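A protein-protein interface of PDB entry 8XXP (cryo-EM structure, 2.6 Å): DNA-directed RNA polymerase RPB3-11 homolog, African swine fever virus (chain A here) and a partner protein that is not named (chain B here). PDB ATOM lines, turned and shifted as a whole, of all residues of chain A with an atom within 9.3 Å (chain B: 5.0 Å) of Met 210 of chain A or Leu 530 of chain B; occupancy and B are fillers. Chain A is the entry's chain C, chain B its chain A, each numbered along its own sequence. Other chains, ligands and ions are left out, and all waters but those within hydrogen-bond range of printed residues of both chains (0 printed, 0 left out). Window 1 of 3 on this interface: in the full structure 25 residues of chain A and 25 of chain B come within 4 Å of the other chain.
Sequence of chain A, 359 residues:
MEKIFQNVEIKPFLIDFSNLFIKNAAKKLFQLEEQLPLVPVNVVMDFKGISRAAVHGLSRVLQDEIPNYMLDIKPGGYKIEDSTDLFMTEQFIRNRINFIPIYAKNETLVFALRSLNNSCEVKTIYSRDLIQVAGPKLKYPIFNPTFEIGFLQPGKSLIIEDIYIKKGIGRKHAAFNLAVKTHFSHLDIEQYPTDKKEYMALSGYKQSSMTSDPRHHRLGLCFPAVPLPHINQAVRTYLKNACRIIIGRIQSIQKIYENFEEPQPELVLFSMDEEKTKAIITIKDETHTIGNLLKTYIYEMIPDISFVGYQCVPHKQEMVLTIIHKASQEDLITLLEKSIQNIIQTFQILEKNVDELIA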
ATOM      1  N   ARG A  52     -14.373  25.469  -0.851  1.00  0.00           N
ATOM      2  CA  ARG A  52     -13.064  25.358  -1.474  1.00  0.00           C
ATOM      3  C   ARG A  52     -12.467  26.730  -1.755  1.00  0.00           C
ATOM      4  O   ARG A  52     -11.245  26.889  -1.746  1.00  0.00           O
ATOM      5  CB  ARG A  52     -13.182  24.533  -2.757  1.00  0.00           C
ATOM      6  CG  ARG A  52     -12.030  24.662  -3.716  1.00  0.00           C
ATOM      7  CD  ARG A  52     -12.228  23.761  -4.913  1.00  0.00           C
ATOM      8  NE  ARG A  52     -13.560  23.892  -5.489  1.00  0.00           N
ATOM      9  CZ  ARG A  52     -14.185  22.928  -6.150  1.00  0.00           C
ATOM     10  NH1 ARG A  52     -13.620  21.752  -6.354  1.00  0.00           N
ATOM     11  NH2 ARG A  52     -15.406  23.152  -6.622  1.00  0.00           N
ATOM     12  N   ILE A 189     -15.007  13.572  -1.167  1.00  0.00           N
ATOM     13  CA  ILE A 189     -15.208  13.021  -2.499  1.00  0.00           C
ATOM     14  C   ILE A 189     -14.454  11.705  -2.572  1.00  0.00           C
ATOM     15  O   ILE A 189     -13.264  11.649  -2.245  1.00  0.00           O
ATOM     16  CB  ILE A 189     -14.740  13.986  -3.604  1.00  0.00           C
ATOM     17  CG1 ILE A 189     -15.325  15.377  -3.387  1.00  0.00           C
ATOM     18  CG2 ILE A 189     -15.155  13.475  -4.965  1.00  0.00           C
ATOM     19  CD1 ILE A 189     -14.895  16.369  -4.421  1.00  0.00           C
ATOM     20  N   TYR A 205     -10.988  11.502  -8.485  1.00  0.00           N
ATOM     21  CA  TYR A 205     -12.241  11.834  -7.827  1.00  0.00           C
ATOM     22  C   TYR A 205     -13.421  11.289  -8.619  1.00  0.00           C
ATOM     23  O   TYR A 205     -13.455  11.366  -9.847  1.00  0.00           O
ATOM     24  CB  TYR A 205     -12.366  13.346  -7.670  1.00  0.00           C
ATOM     25  CG  TYR A 205     -11.484  13.907  -6.591  1.00  0.00           C
ATOM     26  CD1 TYR A 205     -11.574  13.450  -5.291  1.00  0.00           C
ATOM     27  CD2 TYR A 205     -10.550  14.885  -6.875  1.00  0.00           C
ATOM     28  CE1 TYR A 205     -10.770  13.953  -4.307  1.00  0.00           C
ATOM     29  CE2 TYR A 205      -9.742  15.394  -5.895  1.00  0.00           C
ATOM     30  CZ  TYR A 205      -9.854  14.924  -4.614  1.00  0.00           C
ATOM     31  OH  TYR A 205      -9.047  15.427  -3.629  1.00  0.00           O
ATOM     32  N   GLN A 207     -16.427  12.402  -8.644  1.00  0.00           N
ATOM     33  CA  GLN A 207     -17.326  13.454  -9.084  1.00  0.00           C
ATOM     34  C   GLN A 207     -16.567  14.415  -9.977  1.00  0.00           C
ATOM     35  O   GLN A 207     -15.427  14.779  -9.682  1.00  0.00           O
ATOM     36  CB  GLN A 207     -17.917  14.222  -7.906  1.00  0.00           C
ATOM     37  CG  GLN A 207     -18.616  13.365  -6.883  1.00  0.00           C
ATOM     38  CD  GLN A 207     -19.153  14.181  -5.741  1.00  0.00           C
ATOM     39  OE1 GLN A 207     -19.600  15.307  -5.932  1.00  0.00           O
ATOM     40  NE2 GLN A 207     -19.101  13.625  -4.541  1.00  0.00           N
ATOM     41  N   SER A 208     -17.201  14.825 -11.068  1.00  0.00           N
ATOM     42  CA  SER A 208     -16.628  15.866 -11.904  1.00  0.00           C
ATOM     43  C   SER A 208     -16.499  17.155 -11.107  1.00  0.00           C
ATOM     44  O   SER A 208     -17.369  17.497 -10.305  1.00  0.00           O
ATOM     45  CB  SER A 208     -17.498  16.094 -13.135  1.00  0.00           C
ATOM     46  OG  SER A 208     -17.039  17.205 -13.874  1.00  0.00           O
ATOM     47  N   SER A 209     -15.397  17.870 -11.323  1.00  0.00           N
ATOM     48  CA  SER A 209     -15.213  19.147 -10.649  1.00  0.00           C
ATOM     49  C   SER A 209     -16.211  20.192 -11.114  1.00  0.00           C
ATOM     50  O   SER A 209     -16.362  21.220 -10.451  1.00  0.00           O
ATOM     51  CB  SER A 209     -13.791  19.656 -10.856  1.00  0.00           C
ATOM     52  OG  SER A 209     -13.372  19.476 -12.193  1.00  0.00           O
ATOM     53  N   MET A 210     -16.891  19.950 -12.230  1.00  0.00           N
ATOM     54  CA  MET A 210     -17.920  20.850 -12.720  1.00  0.00           C
ATOM     55  C   MET A 210     -19.245  20.685 -11.997  1.00  0.00           C
ATOM     56  O   MET A 210     -20.142  21.507 -12.189  1.00  0.00           O
ATOM     57  CB  MET A 210     -18.118  20.641 -14.218  1.00  0.00           C
ATOM     58  CG  MET A 210     -16.850  20.797 -15.020  1.00  0.00           C
ATOM     59  SD  MET A 210     -17.109  21.663 -16.569  1.00  0.00           S
ATOM     60  CE  MET A 210     -16.974  23.366 -16.042  1.00  0.00           C
ATOM     61  N   THR A 211     -19.389  19.653 -11.173  1.00  0.00           N
ATOM     62  CA  THR A 211     -20.595  19.445 -10.386  1.00  0.00           C
ATOM     63  C   THR A 211     -20.340  19.276  -8.899  1.00  0.00           C
ATOM     64  O   THR A 211     -21.282  19.431  -8.116  1.00  0.00           O
ATOM     65  CB  THR A 211     -21.362  18.213 -10.886  1.00  0.00           C
ATOM     66  OG1 THR A 211     -20.538  17.052 -10.754  1.00  0.00           O
ATOM     67  CG2 THR A 211     -21.754  18.380 -12.334  1.00  0.00           C
ATOM     68  N   SER A 212     -19.120  18.961  -8.483  1.00  0.00           N
ATOM     69  CA  SER A 212     -18.828  18.723  -7.080  1.00  0.00           C
ATOM     70  C   SER A 212     -18.731  20.031  -6.306  1.00  0.00           C
ATOM     71  O   SER A 212     -18.300  21.060  -6.828  1.00  0.00           O
ATOM     72  CB  SER A 212     -17.526  17.945  -6.929  1.00  0.00           C
ATOM     73  OG  SER A 212     -16.427  18.733  -7.332  1.00  0.00           O
ATOM     74  N   ASP A 213     -19.146  19.978  -5.046  1.00  0.00           N
ATOM     75  CA  ASP A 213     -19.028  21.094  -4.112  1.00  0.00           C
ATOM     76  C   ASP A 213     -18.430  20.554  -2.822  1.00  0.00           C
ATOM     77  O   ASP A 213     -19.143  20.332  -1.837  1.00  0.00           O
ATOM     78  CB  ASP A 213     -20.380  21.759  -3.863  1.00  0.00           C
ATOM     79  CG  ASP A 213     -20.296  22.884  -2.862  1.00  0.00           C
ATOM     80  OD1 ASP A 213     -19.241  23.545  -2.799  1.00  0.00           O
ATOM     81  OD2 ASP A 213     -21.280  23.104  -2.126  1.00  0.00           O
ATOM     82  N   PRO A 214     -17.122  20.312  -2.797  1.00  0.00           N
ATOM     83  CA  PRO A 214     -16.513  19.718  -1.606  1.00  0.00           C
ATOM     84  C   PRO A 214     -16.464  20.703  -0.451  1.00  0.00           C
ATOM     85  O   PRO A 214     -16.238  21.901  -0.636  1.00  0.00           O
ATOM     86  CB  PRO A 214     -15.110  19.339  -2.083  1.00  0.00           C
ATOM     87  CG  PRO A 214     -14.830  20.284  -3.179  1.00  0.00           C
ATOM     88  CD  PRO A 214     -16.125  20.607  -3.839  1.00  0.00           C
ATOM     89  N   LYS A 295     -17.163  35.618  -5.312  1.00  0.00           N
ATOM     90  CA  LYS A 295     -18.113  34.915  -6.165  1.00  0.00           C
ATOM     91  C   LYS A 295     -18.756  33.757  -5.420  1.00  0.00           C
ATOM     92  O   LYS A 295     -19.979  33.580  -5.462  1.00  0.00           O
ATOM     93  CB  LYS A 295     -17.422  34.421  -7.433  1.00  0.00           C
ATOM     94  CG  LYS A 295     -18.346  33.682  -8.373  1.00  0.00           C
ATOM     95  CD  LYS A 295     -17.587  33.023  -9.497  1.00  0.00           C
ATOM     96  CE  LYS A 295     -16.754  31.867  -8.998  1.00  0.00           C
ATOM     97  NZ  LYS A 295     -16.333  30.984 -10.116  1.00  0.00           N
ATOM     98  N   TYR A 299     -22.712  33.718  -4.405  1.00  0.00           N
ATOM     99  CA  TYR A 299     -23.509  32.617  -4.923  1.00  0.00           C
ATOM    100  C   TYR A 299     -24.175  31.833  -3.803  1.00  0.00           C
ATOM    101  O   TYR A 299     -25.351  31.467  -3.903  1.00  0.00           O
ATOM    102  CB  TYR A 299     -22.611  31.713  -5.753  1.00  0.00           C
ATOM    103  CG  TYR A 299     -23.305  30.566  -6.417  1.00  0.00           C
ATOM    104  CD1 TYR A 299     -24.319  30.783  -7.330  1.00  0.00           C
ATOM    105  CD2 TYR A 299     -22.924  29.266  -6.157  1.00  0.00           C
ATOM    106  CE1 TYR A 299     -24.939  29.742  -7.946  1.00  0.00           C
ATOM    107  CE2 TYR A 299     -23.541  28.221  -6.768  1.00  0.00           C
ATOM    108  CZ  TYR A 299     -24.544  28.466  -7.663  1.00  0.00           C
ATOM    109  OH  TYR A 299     -25.153  27.418  -8.281  1.00  0.00           O
ATOM    110  N   PHE A 307     -26.614  36.228 -12.432  1.00  0.00           N
ATOM    111  CA  PHE A 307     -25.239  35.956 -12.822  1.00  0.00           C
ATOM    112  C   PHE A 307     -24.301  36.501 -11.758  1.00  0.00           C
ATOM    113  O   PHE A 307     -24.508  37.602 -11.250  1.00  0.00           O
ATOM    114  CB  PHE A 307     -24.899  36.579 -14.179  1.00  0.00           C
ATOM    115  CG  PHE A 307     -23.476  36.362 -14.599  1.00  0.00           C
ATOM    116  CD1 PHE A 307     -23.078  35.158 -15.142  1.00  0.00           C
ATOM    117  CD2 PHE A 307     -22.533  37.358 -14.438  1.00  0.00           C
ATOM    118  CE1 PHE A 307     -21.773  34.954 -15.517  1.00  0.00           C
ATOM    119  CE2 PHE A 307     -21.228  37.155 -14.815  1.00  0.00           C
ATOM    120  CZ  PHE A 307     -20.849  35.952 -15.354  1.00  0.00           C
ATOM    121  N   VAL A 308     -23.280  35.720 -11.424  1.00  0.00           N
ATOM    122  CA  VAL A 308     -22.155  36.195 -10.628  1.00  0.00           C
ATOM    123  C   VAL A 308     -20.883  35.622 -11.230  1.00  0.00           C
ATOM    124  O   VAL A 308     -20.820  34.433 -11.553  1.00  0.00           O
ATOM    125  CB  VAL A 308     -22.283  35.821  -9.136  1.00  0.00           C
ATOM    126  CG1 VAL A 308     -22.440  34.325  -8.949  1.00  0.00           C
ATOM    127  CG2 VAL A 308     -21.097  36.342  -8.358  1.00  0.00           C
ATOM    128  N   GLY A 309     -19.882  36.468 -11.409  1.00  0.00           N
ATOM    129  CA  GLY A 309     -18.625  36.014 -11.957  1.00  0.00           C
ATOM    130  C   GLY A 309     -17.584  37.100 -11.864  1.00  0.00           C
ATOM    131  O   GLY A 309     -17.903  38.289 -11.784  1.00  0.00           O
ATOM    132  N   TYR A 310     -16.330  36.672 -11.884  1.00  0.00           N
ATOM    133  CA  TYR A 310     -15.194  37.570 -11.798  1.00  0.00           C
ATOM    134  C   TYR A 310     -14.203  37.228 -12.897  1.00  0.00           C
ATOM    135  O   TYR A 310     -14.170  36.108 -13.405  1.00  0.00           O
ATOM    136  CB  TYR A 310     -14.514  37.491 -10.423  1.00  0.00           C
ATOM    137  CG  TYR A 310     -13.588  36.307 -10.265  1.00  0.00           C
ATOM    138  CD1 TYR A 310     -14.086  35.049  -9.991  1.00  0.00           C
ATOM    139  CD2 TYR A 310     -12.219  36.452 -10.398  1.00  0.00           C
ATOM    140  CE1 TYR A 310     -13.252  33.972  -9.855  1.00  0.00           C
ATOM    141  CE2 TYR A 310     -11.380  35.385 -10.265  1.00  0.00           C
ATOM    142  CZ  TYR A 310     -11.897  34.144  -9.993  1.00  0.00           C
ATOM    143  OH  TYR A 310     -11.056  33.068  -9.854  1.00  0.00           O
ATOM    144  N   LEU B 510     -16.421  20.432 -24.536  1.00  0.00           N
ATOM    145  CA  LEU B 510     -17.570  21.113 -23.960  1.00  0.00           C
ATOM    146  C   LEU B 510     -18.879  20.527 -24.469  1.00  0.00           C
ATOM    147  O   LEU B 510     -19.811  20.315 -23.689  1.00  0.00           O
ATOM    148  CB  LEU B 510     -17.488  22.606 -24.268  1.00  0.00           C
ATOM    149  CG  LEU B 510     -18.701  23.492 -24.000  1.00  0.00           C
ATOM    150  CD1 LEU B 510     -19.121  23.412 -22.556  1.00  0.00           C
ATOM    151  CD2 LEU B 510     -18.370  24.908 -24.367  1.00  0.00           C
ATOM    152  N   VAL B 521     -22.226  17.267 -17.842  1.00  0.00           N
ATOM    153  CA  VAL B 521     -23.048  18.258 -17.167  1.00  0.00           C
ATOM    154  C   VAL B 521     -22.173  19.092 -16.248  1.00  0.00           C
ATOM    155  O   VAL B 521     -21.122  18.648 -15.778  1.00  0.00           O
ATOM    156  CB  VAL B 521     -24.193  17.604 -16.368  1.00  0.00           C
ATOM    157  CG1 VAL B 521     -25.225  17.047 -17.302  1.00  0.00           C
ATOM    158  CG2 VAL B 521     -23.656  16.519 -15.465  1.00  0.00           C
ATOM    159  N   MET B 522     -22.621  20.316 -15.996  1.00  0.00           N
ATOM    160  CA  MET B 522     -22.007  21.188 -15.012  1.00  0.00           C
ATOM    161  C   MET B 522     -23.114  21.849 -14.212  1.00  0.00           C
ATOM    162  O   MET B 522     -24.235  21.999 -14.695  1.00  0.00           O
ATOM    163  CB  MET B 522     -21.110  22.240 -15.670  1.00  0.00           C
ATOM    164  CG  MET B 522     -21.855  23.252 -16.509  1.00  0.00           C
ATOM    165  SD  MET B 522     -20.828  23.980 -17.788  1.00  0.00           S
ATOM    166  CE  MET B 522     -20.923  22.711 -19.036  1.00  0.00           C
ATOM    167  N   ASN B 523     -22.800  22.228 -12.980  1.00  0.00           N
ATOM    168  CA  ASN B 523     -23.777  22.897 -12.141  1.00  0.00           C
ATOM    169  C   ASN B 523     -23.842  24.379 -12.501  1.00  0.00           C
ATOM    170  O   ASN B 523     -23.119  24.866 -13.369  1.00  0.00           O
ATOM    171  CB  ASN B 523     -23.452  22.673 -10.665  1.00  0.00           C
ATOM    172  CG  ASN B 523     -22.214  23.410 -10.217  1.00  0.00           C
ATOM    173  OD1 ASN B 523     -22.262  24.595  -9.923  1.00  0.00           O
ATOM    174  ND2 ASN B 523     -21.102  22.703 -10.133  1.00  0.00           N
ATOM    175  N   HIS B 526     -20.560  26.503 -12.289  1.00  0.00           N
ATOM    176  CA  HIS B 526     -19.602  26.304 -13.365  1.00  0.00           C
ATOM    177  C   HIS B 526     -20.152  26.733 -14.713  1.00  0.00           C
ATOM    178  O   HIS B 526     -19.383  27.156 -15.578  1.00  0.00           O
ATOM    179  CB  HIS B 526     -19.161  24.847 -13.398  1.00  0.00           C
ATOM    180  CG  HIS B 526     -18.236  24.488 -12.283  1.00  0.00           C
ATOM    181  ND1 HIS B 526     -18.674  24.278 -10.997  1.00  0.00           N
ATOM    182  CD2 HIS B 526     -16.894  24.337 -12.253  1.00  0.00           C
ATOM    183  CE1 HIS B 526     -17.645  23.994 -10.224  1.00  0.00           C
ATOM    184  NE2 HIS B 526     -16.551  24.021 -10.963  1.00  0.00           N
ATOM    185  N   ALA B 527     -21.465  26.625 -14.918  1.00  0.00           N
ATOM    186  CA  ALA B 527     -22.063  27.182 -16.124  1.00  0.00           C
ATOM    187  C   ALA B 527     -21.913  28.695 -16.156  1.00  0.00           C
ATOM    188  O   ALA B 527     -21.593  29.271 -17.202  1.00  0.00           O
ATOM    189  CB  ALA B 527     -23.533  26.787 -16.214  1.00  0.00           C
ATOM    190  N   MET B 528     -22.142  29.358 -15.021  1.00  0.00           N
ATOM    191  CA  MET B 528     -21.891  30.791 -14.942  1.00  0.00           C
ATOM    192  C   MET B 528     -20.419  31.100 -15.161  1.00  0.00           C
ATOM    193  O   MET B 528     -20.078  32.087 -15.820  1.00  0.00           O
ATOM    194  CB  MET B 528     -22.350  31.341 -13.592  1.00  0.00           C
ATOM    195  CG  MET B 528     -23.791  31.790 -13.545  1.00  0.00           C
ATOM    196  SD  MET B 528     -24.344  32.305 -11.916  1.00  0.00           S
ATOM    197  CE  MET B 528     -23.329  31.272 -10.875  1.00  0.00           C
ATOM    198  N   GLY B 529     -19.533  30.268 -14.616  1.00  0.00           N
ATOM    199  CA  GLY B 529     -18.109  30.512 -14.719  1.00  0.00           C
ATOM    200  C   GLY B 529     -17.557  30.391 -16.119  1.00  0.00           C
ATOM    201  O   GLY B 529     -16.450  30.867 -16.378  1.00  0.00           O
ATOM    202  N   LEU B 530     -18.294  29.750 -17.022  1.00  0.00           N
ATOM    203  CA  LEU B 530     -17.855  29.663 -18.407  1.00  0.00           C
ATOM    204  C   LEU B 530     -17.978  31.001 -19.114  1.00  0.00           C
ATOM    205  O   LEU B 530     -17.230  31.273 -20.057  1.00  0.00           O
ATOM    206  CB  LEU B 530     -18.663  28.601 -19.141  1.00  0.00           C
ATOM    207  CG  LEU B 530     -17.981  27.260 -19.389  1.00  0.00           C
ATOM    208  CD1 LEU B 530     -17.346  26.744 -18.127  1.00  0.00           C
ATOM    209  CD2 LEU B 530     -18.983  26.273 -19.921  1.00  0.00           C
ATOM    210  N   PHE B 531     -18.902  31.846 -18.670  1.00  0.00           N
ATOM    211  CA  PHE B 531     -19.191  33.119 -19.308  1.00  0.00           C
ATOM    212  C   PHE B 531     -18.465  34.281 -18.651  1.00  0.00           C
ATOM    213  O   PHE B 531     -18.737  35.436 -18.987  1.00  0.00           O
ATOM    214  CB  PHE B 531     -20.695  33.368 -19.301  1.00  0.00           C
ATOM    215  CG  PHE B 531     -21.453  32.488 -20.242  1.00  0.00           C
ATOM    216  CD1 PHE B 531     -21.668  32.874 -21.549  1.00  0.00           C
ATOM    217  CD2 PHE B 531     -21.938  31.265 -19.823  1.00  0.00           C
ATOM    218  CE1 PHE B 531     -22.361  32.063 -22.411  1.00  0.00           C
ATOM    219  CE2 PHE B 531     -22.628  30.453 -20.682  1.00  0.00           C
ATOM    220  CZ  PHE B 531     -22.841  30.852 -21.977  1.00  0.00           C
ATOM    221  N   GLN B 532     -17.555  34.000 -17.721  1.00  0.00           N
ATOM    222  CA  GLN B 532     -16.881  35.066 -16.991  1.00  0.00           C
ATOM    223  C   GLN B 532     -16.030  35.926 -17.914  1.00  0.00           C
ATOM    224  O   GLN B 532     -15.995  37.151 -17.776  1.00  0.00           O
ATOM    225  CB  GLN B 532     -16.015  34.470 -15.889  1.00  0.00           C
ATOM    226  CG  GLN B 532     -16.781  33.987 -14.697  1.00  0.00           C
ATOM    227  CD  GLN B 532     -15.882  33.387 -13.654  1.00  0.00           C
ATOM    228  OE1 GLN B 532     -14.846  32.813 -13.965  1.00  0.00           O
ATOM    229  NE2 GLN B 532     -16.269  33.525 -12.402  1.00  0.00           N
ATOM    230  N   THR B 533     -15.329  35.301 -18.852  1.00  0.00           N
ATOM    231  CA  THR B 533     -14.334  35.980 -19.664  1.00  0.00           C
ATOM    232  C   THR B 533     -14.796  36.241 -21.088  1.00  0.00           C
ATOM    233  O   THR B 533     -14.003  36.716 -21.904  1.00  0.00           O
ATOM    234  CB  THR B 533     -13.043  35.167 -19.677  1.00  0.00           C
ATOM    235  OG1 THR B 533     -13.331  33.832 -20.098  1.00  0.00           O
ATOM    236  CG2 THR B 533     -12.433  35.125 -18.293  1.00  0.00           C
ATOM    237  N   THR B 534     -16.058  35.956 -21.406  1.00  0.00           N
ATOM    238  CA  THR B 534     -16.537  36.151 -22.768  1.00  0.00           C
ATOM    239  C   THR B 534     -16.635  37.618 -23.143  1.00  0.00           C
ATOM    240  O   THR B 534     -16.768  37.931 -24.329  1.00  0.00           O
ATOM    241  CB  THR B 534     -17.896  35.485 -22.956  1.00  0.00           C
ATOM    242  OG1 THR B 534     -18.828  36.033 -22.021  1.00  0.00           O
ATOM    243  CG2 THR B 534     -17.789  34.006 -22.728  1.00  0.00           C
ATOM    244  N   VAL B 555     -25.172  25.375 -22.514  1.00  0.00           N
ATOM    245  CA  VAL B 555     -24.441  26.617 -22.290  1.00  0.00           C
ATOM    246  C   VAL B 555     -23.953  27.205 -23.605  1.00  0.00           C
ATOM    247  O   VAL B 555     -23.855  28.428 -23.743  1.00  0.00           O
ATOM    248  CB  VAL B 555     -23.288  26.405 -21.291  1.00  0.00           C
ATOM    249  CG1 VAL B 555     -23.826  25.901 -19.973  1.00  0.00           C
ATOM    250  CG2 VAL B 555     -22.260  25.454 -21.840  1.00  0.00           C
ATOM    251  N   GLN B 638     -13.660  31.571 -25.443  1.00  0.00           N
ATOM    252  CA  GLN B 638     -13.624  31.676 -23.991  1.00  0.00           C
ATOM    253  C   GLN B 638     -14.411  30.555 -23.334  1.00  0.00           C
ATOM    254  O   GLN B 638     -13.983  30.011 -22.314  1.00  0.00           O
ATOM    255  CB  GLN B 638     -14.157  33.034 -23.547  1.00  0.00           C
ATOM    256  CG  GLN B 638     -13.300  34.198 -23.970  1.00  0.00           C
ATOM    257  CD  GLN B 638     -11.828  33.929 -23.787  1.00  0.00           C
ATOM    258  OE1 GLN B 638     -11.374  33.625 -22.690  1.00  0.00           O
ATOM    259  NE2 GLN B 638     -11.072  34.034 -24.867  1.00  0.00           N
ATOM    260  N   LEU B 639     -15.563  30.199 -23.899  1.00  0.00           N
ATOM    261  CA  LEU B 639     -16.330  29.077 -23.372  1.00  0.00           C
ATOM    262  C   LEU B 639     -15.536  27.784 -23.442  1.00  0.00           C
ATOM    263  O   LEU B 639     -15.507  27.012 -22.480  1.00  0.00           O
ATOM    264  CB  LEU B 639     -17.639  28.933 -24.141  1.00  0.00           C
ATOM    265  CG  LEU B 639     -18.933  29.263 -23.411  1.00  0.00           C
ATOM    266  CD1 LEU B 639     -18.994  30.725 -23.079  1.00  0.00           C
ATOM    267  CD2 LEU B 639     -20.099  28.880 -24.283  1.00  0.00           C
ATOM    268  N   ASN B 642     -12.592  28.105 -20.903  1.00  0.00           N
ATOM    269  CA  ASN B 642     -13.044  28.029 -19.521  1.00  0.00           C
ATOM    270  C   ASN B 642     -13.549  26.639 -19.173  1.00  0.00           C
ATOM    271  O   ASN B 642     -13.541  26.254 -18.000  1.00  0.00           O
ATOM    272  CB  ASN B 642     -14.134  29.061 -19.261  1.00  0.00           C
ATOM    273  CG  ASN B 642     -13.620  30.474 -19.319  1.00  0.00           C
ATOM    274  OD1 ASN B 642     -12.419  30.707 -19.279  1.00  0.00           O
ATOM    275  ND2 ASN B 642     -14.527  31.429 -19.413  1.00  0.00           N
ATOM    276  N   TYR B 643     -14.006  25.878 -20.165  1.00  0.00           N
ATOM    277  CA  TYR B 643     -14.413  24.505 -19.903  1.00  0.00           C
ATOM    278  C   TYR B 643     -13.209  23.623 -19.614  1.00  0.00           C
ATOM    279  O   TYR B 643     -13.208  22.857 -18.646  1.00  0.00           O
ATOM    280  CB  TYR B 643     -15.208  23.952 -21.082  1.00  0.00           C
ATOM    281  CG  TYR B 643     -15.659  22.535 -20.861  1.00  0.00           C
ATOM    282  CD1 TYR B 643     -16.806  22.262 -20.146  1.00  0.00           C
ATOM    283  CD2 TYR B 643     -14.923  21.470 -21.346  1.00  0.00           C
ATOM    284  CE1 TYR B 643     -17.216  20.976 -19.935  1.00  0.00           C
ATOM    285  CE2 TYR B 643     -15.324  20.184 -21.132  1.00  0.00           C
ATOM    286  CZ  TYR B 643     -16.470  19.941 -20.428  1.00  0.00           C
ATOM    287  OH  TYR B 643     -16.875  18.652 -20.217  1.00  0.00           O
ATOM    288  N   ASN B 646     -11.629  23.387 -16.264  1.00  0.00           N
ATOM    289  CA  ASN B 646     -12.082  22.361 -15.339  1.00  0.00           C
ATOM    290  C   ASN B 646     -11.927  20.958 -15.890  1.00  0.00           C
ATOM    291  O   ASN B 646     -11.576  20.047 -15.147  1.00  0.00           O
ATOM    292  CB  ASN B 646     -13.549  22.590 -14.975  1.00  0.00           C
ATOM    293  CG  ASN B 646     -13.711  23.390 -13.718  1.00  0.00           C
ATOM    294  OD1 ASN B 646     -13.820  22.834 -12.631  1.00  0.00           O
ATOM    295  ND2 ASN B 646     -13.724  24.707 -13.852  1.00  0.00           N
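The side-chain amide nitrogen (ND2) of Asn 523 of chain B lies within hydrogen-bond range of the backbone carbonyl oxygen (O) of Met 210 of chain A (2.6 Å).
The backbone carbonyl oxygen of Ser 209 of chain A is in hydrogen-bond range of a ring nitrogen (NE2) of His 526 of chain B (2.9 Å).
OD1 of Asn 646 of chain B sits at hydrogen-bond distance from OG of Ser 209 of chain A (3.4 Å).
NE2 of Gln 532 of chain B sits close to NZ of Lys 295 of chain A (3.4 Å).
N of Val 308 of chain A lies within hydrogen-bond range of SD of Met 528 of chain B (3.6 Å).
The backbone carbonyl oxygen (O) of Met 210 of chain A is in hydrogen-bond range of a ring nitrogen (ND1) of His 526 of chain B (3.4 Å).
The backbone NH (N) of Tyr 310 of chain A sits close to the side-chain amide nitrogen (NE2) of Gln 532 of chain B (3.2 Å).
Met 210 of chain A touches Val 521 of chain B.
Met 210 of chain A touches Met 522 of chain B.
CE of Met 210 of chain A touches CD1 of Leu 530 of chain B, at 3.99 Å.
Met 210 of chain A touches Asn 646 of chain B.
O of Val 521 of chain B touches CG2 of Thr 211 of chain A, at 3.5 Å.
CG2 of Thr 211 of chain A touches CA of Met 522 of chain B, 3.9 Å away.
Thr 211 of chain A touches Asn 523 of chain B.
Tyr 299 of chain A touches Met 528 of chain B (CE1 to CE, 3.7 Å).
Phe 307 of chain A touches Met 528 of chain B (CE1 to O, 3.3 Å).
Gly 309 of chain A touches Gln 532 of chain B.
Hydrophobic or aromatic side chains of chain B that line the printed part of chain A: Met 522, His 526, Met 528, Leu 530 and Tyr 643.
Of the 17 printed residues of chain A, 9 touch a printed residue of chain B.
ND1 of His 526 of chain B lies within hydrogen-bond range of ND2 of Asn 523 of chain B, 3.0 Å away.
The backbone carbonyl oxygen (O) of Gly 529 of chain B lies close to the side-chain amide oxygen (OE1) of Gln 532 of chain B (3.5 Å).
O of Leu 530 of chain B sits at hydrogen-bond distance from ND2 of Asn 642 of chain B (2.8 Å).
The backbone NH (N) of Met 210 of chain A lies close to the side-chain hydroxyl (OG) of Ser 208 of chain A.
O of Ser 208 of chain A sits at hydrogen-bond distance from OG1 of Thr 211 of chain A, 3.2 Å away.
The side-chain amide oxygen (OD1) of Asn 646 of chain B lies within hydrogen-bond range of a ring nitrogen (NE2) of His 526 of chain B (3.4 Å).
Printed residues of chain A within 4 Å of Leu 530 of chain B: Met 210.
Met 522 of chain B touches just these residues of chain A: Met 210 and Thr 211.
Of the printed residues of chain A, His 526 of chain B touches Ser 209 and Met 210.
No residue of chain A comes within 4 Å of Leu 639 of chain B.
Of the printed residues of chain B, Tyr 310 of chain A touches Gln 532 (3.2 Å).
Of the printed residues of chain B, Ser 209 of chain A touches His 526 (2.9 Å) and Asn 646 (3.4 Å).
Printed residues of chain B within 4 Å of Tyr 299 of chain A: Met 528.
Of the printed residues of chain B, Val 308 of chain A touches Met 528.
Of the printed residues of chain B, Thr 211 of chain A touches Val 521, Met 522 and Asn 523.
Val 555 of chain B touches none of the printed residues of chain A.
Ser 212 of chain A touches none of the printed residues of chain B.
The nearest printed residue of chain B that does not touch Met 210 of chain A is Asn 642 of chain B (4.9 Å).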
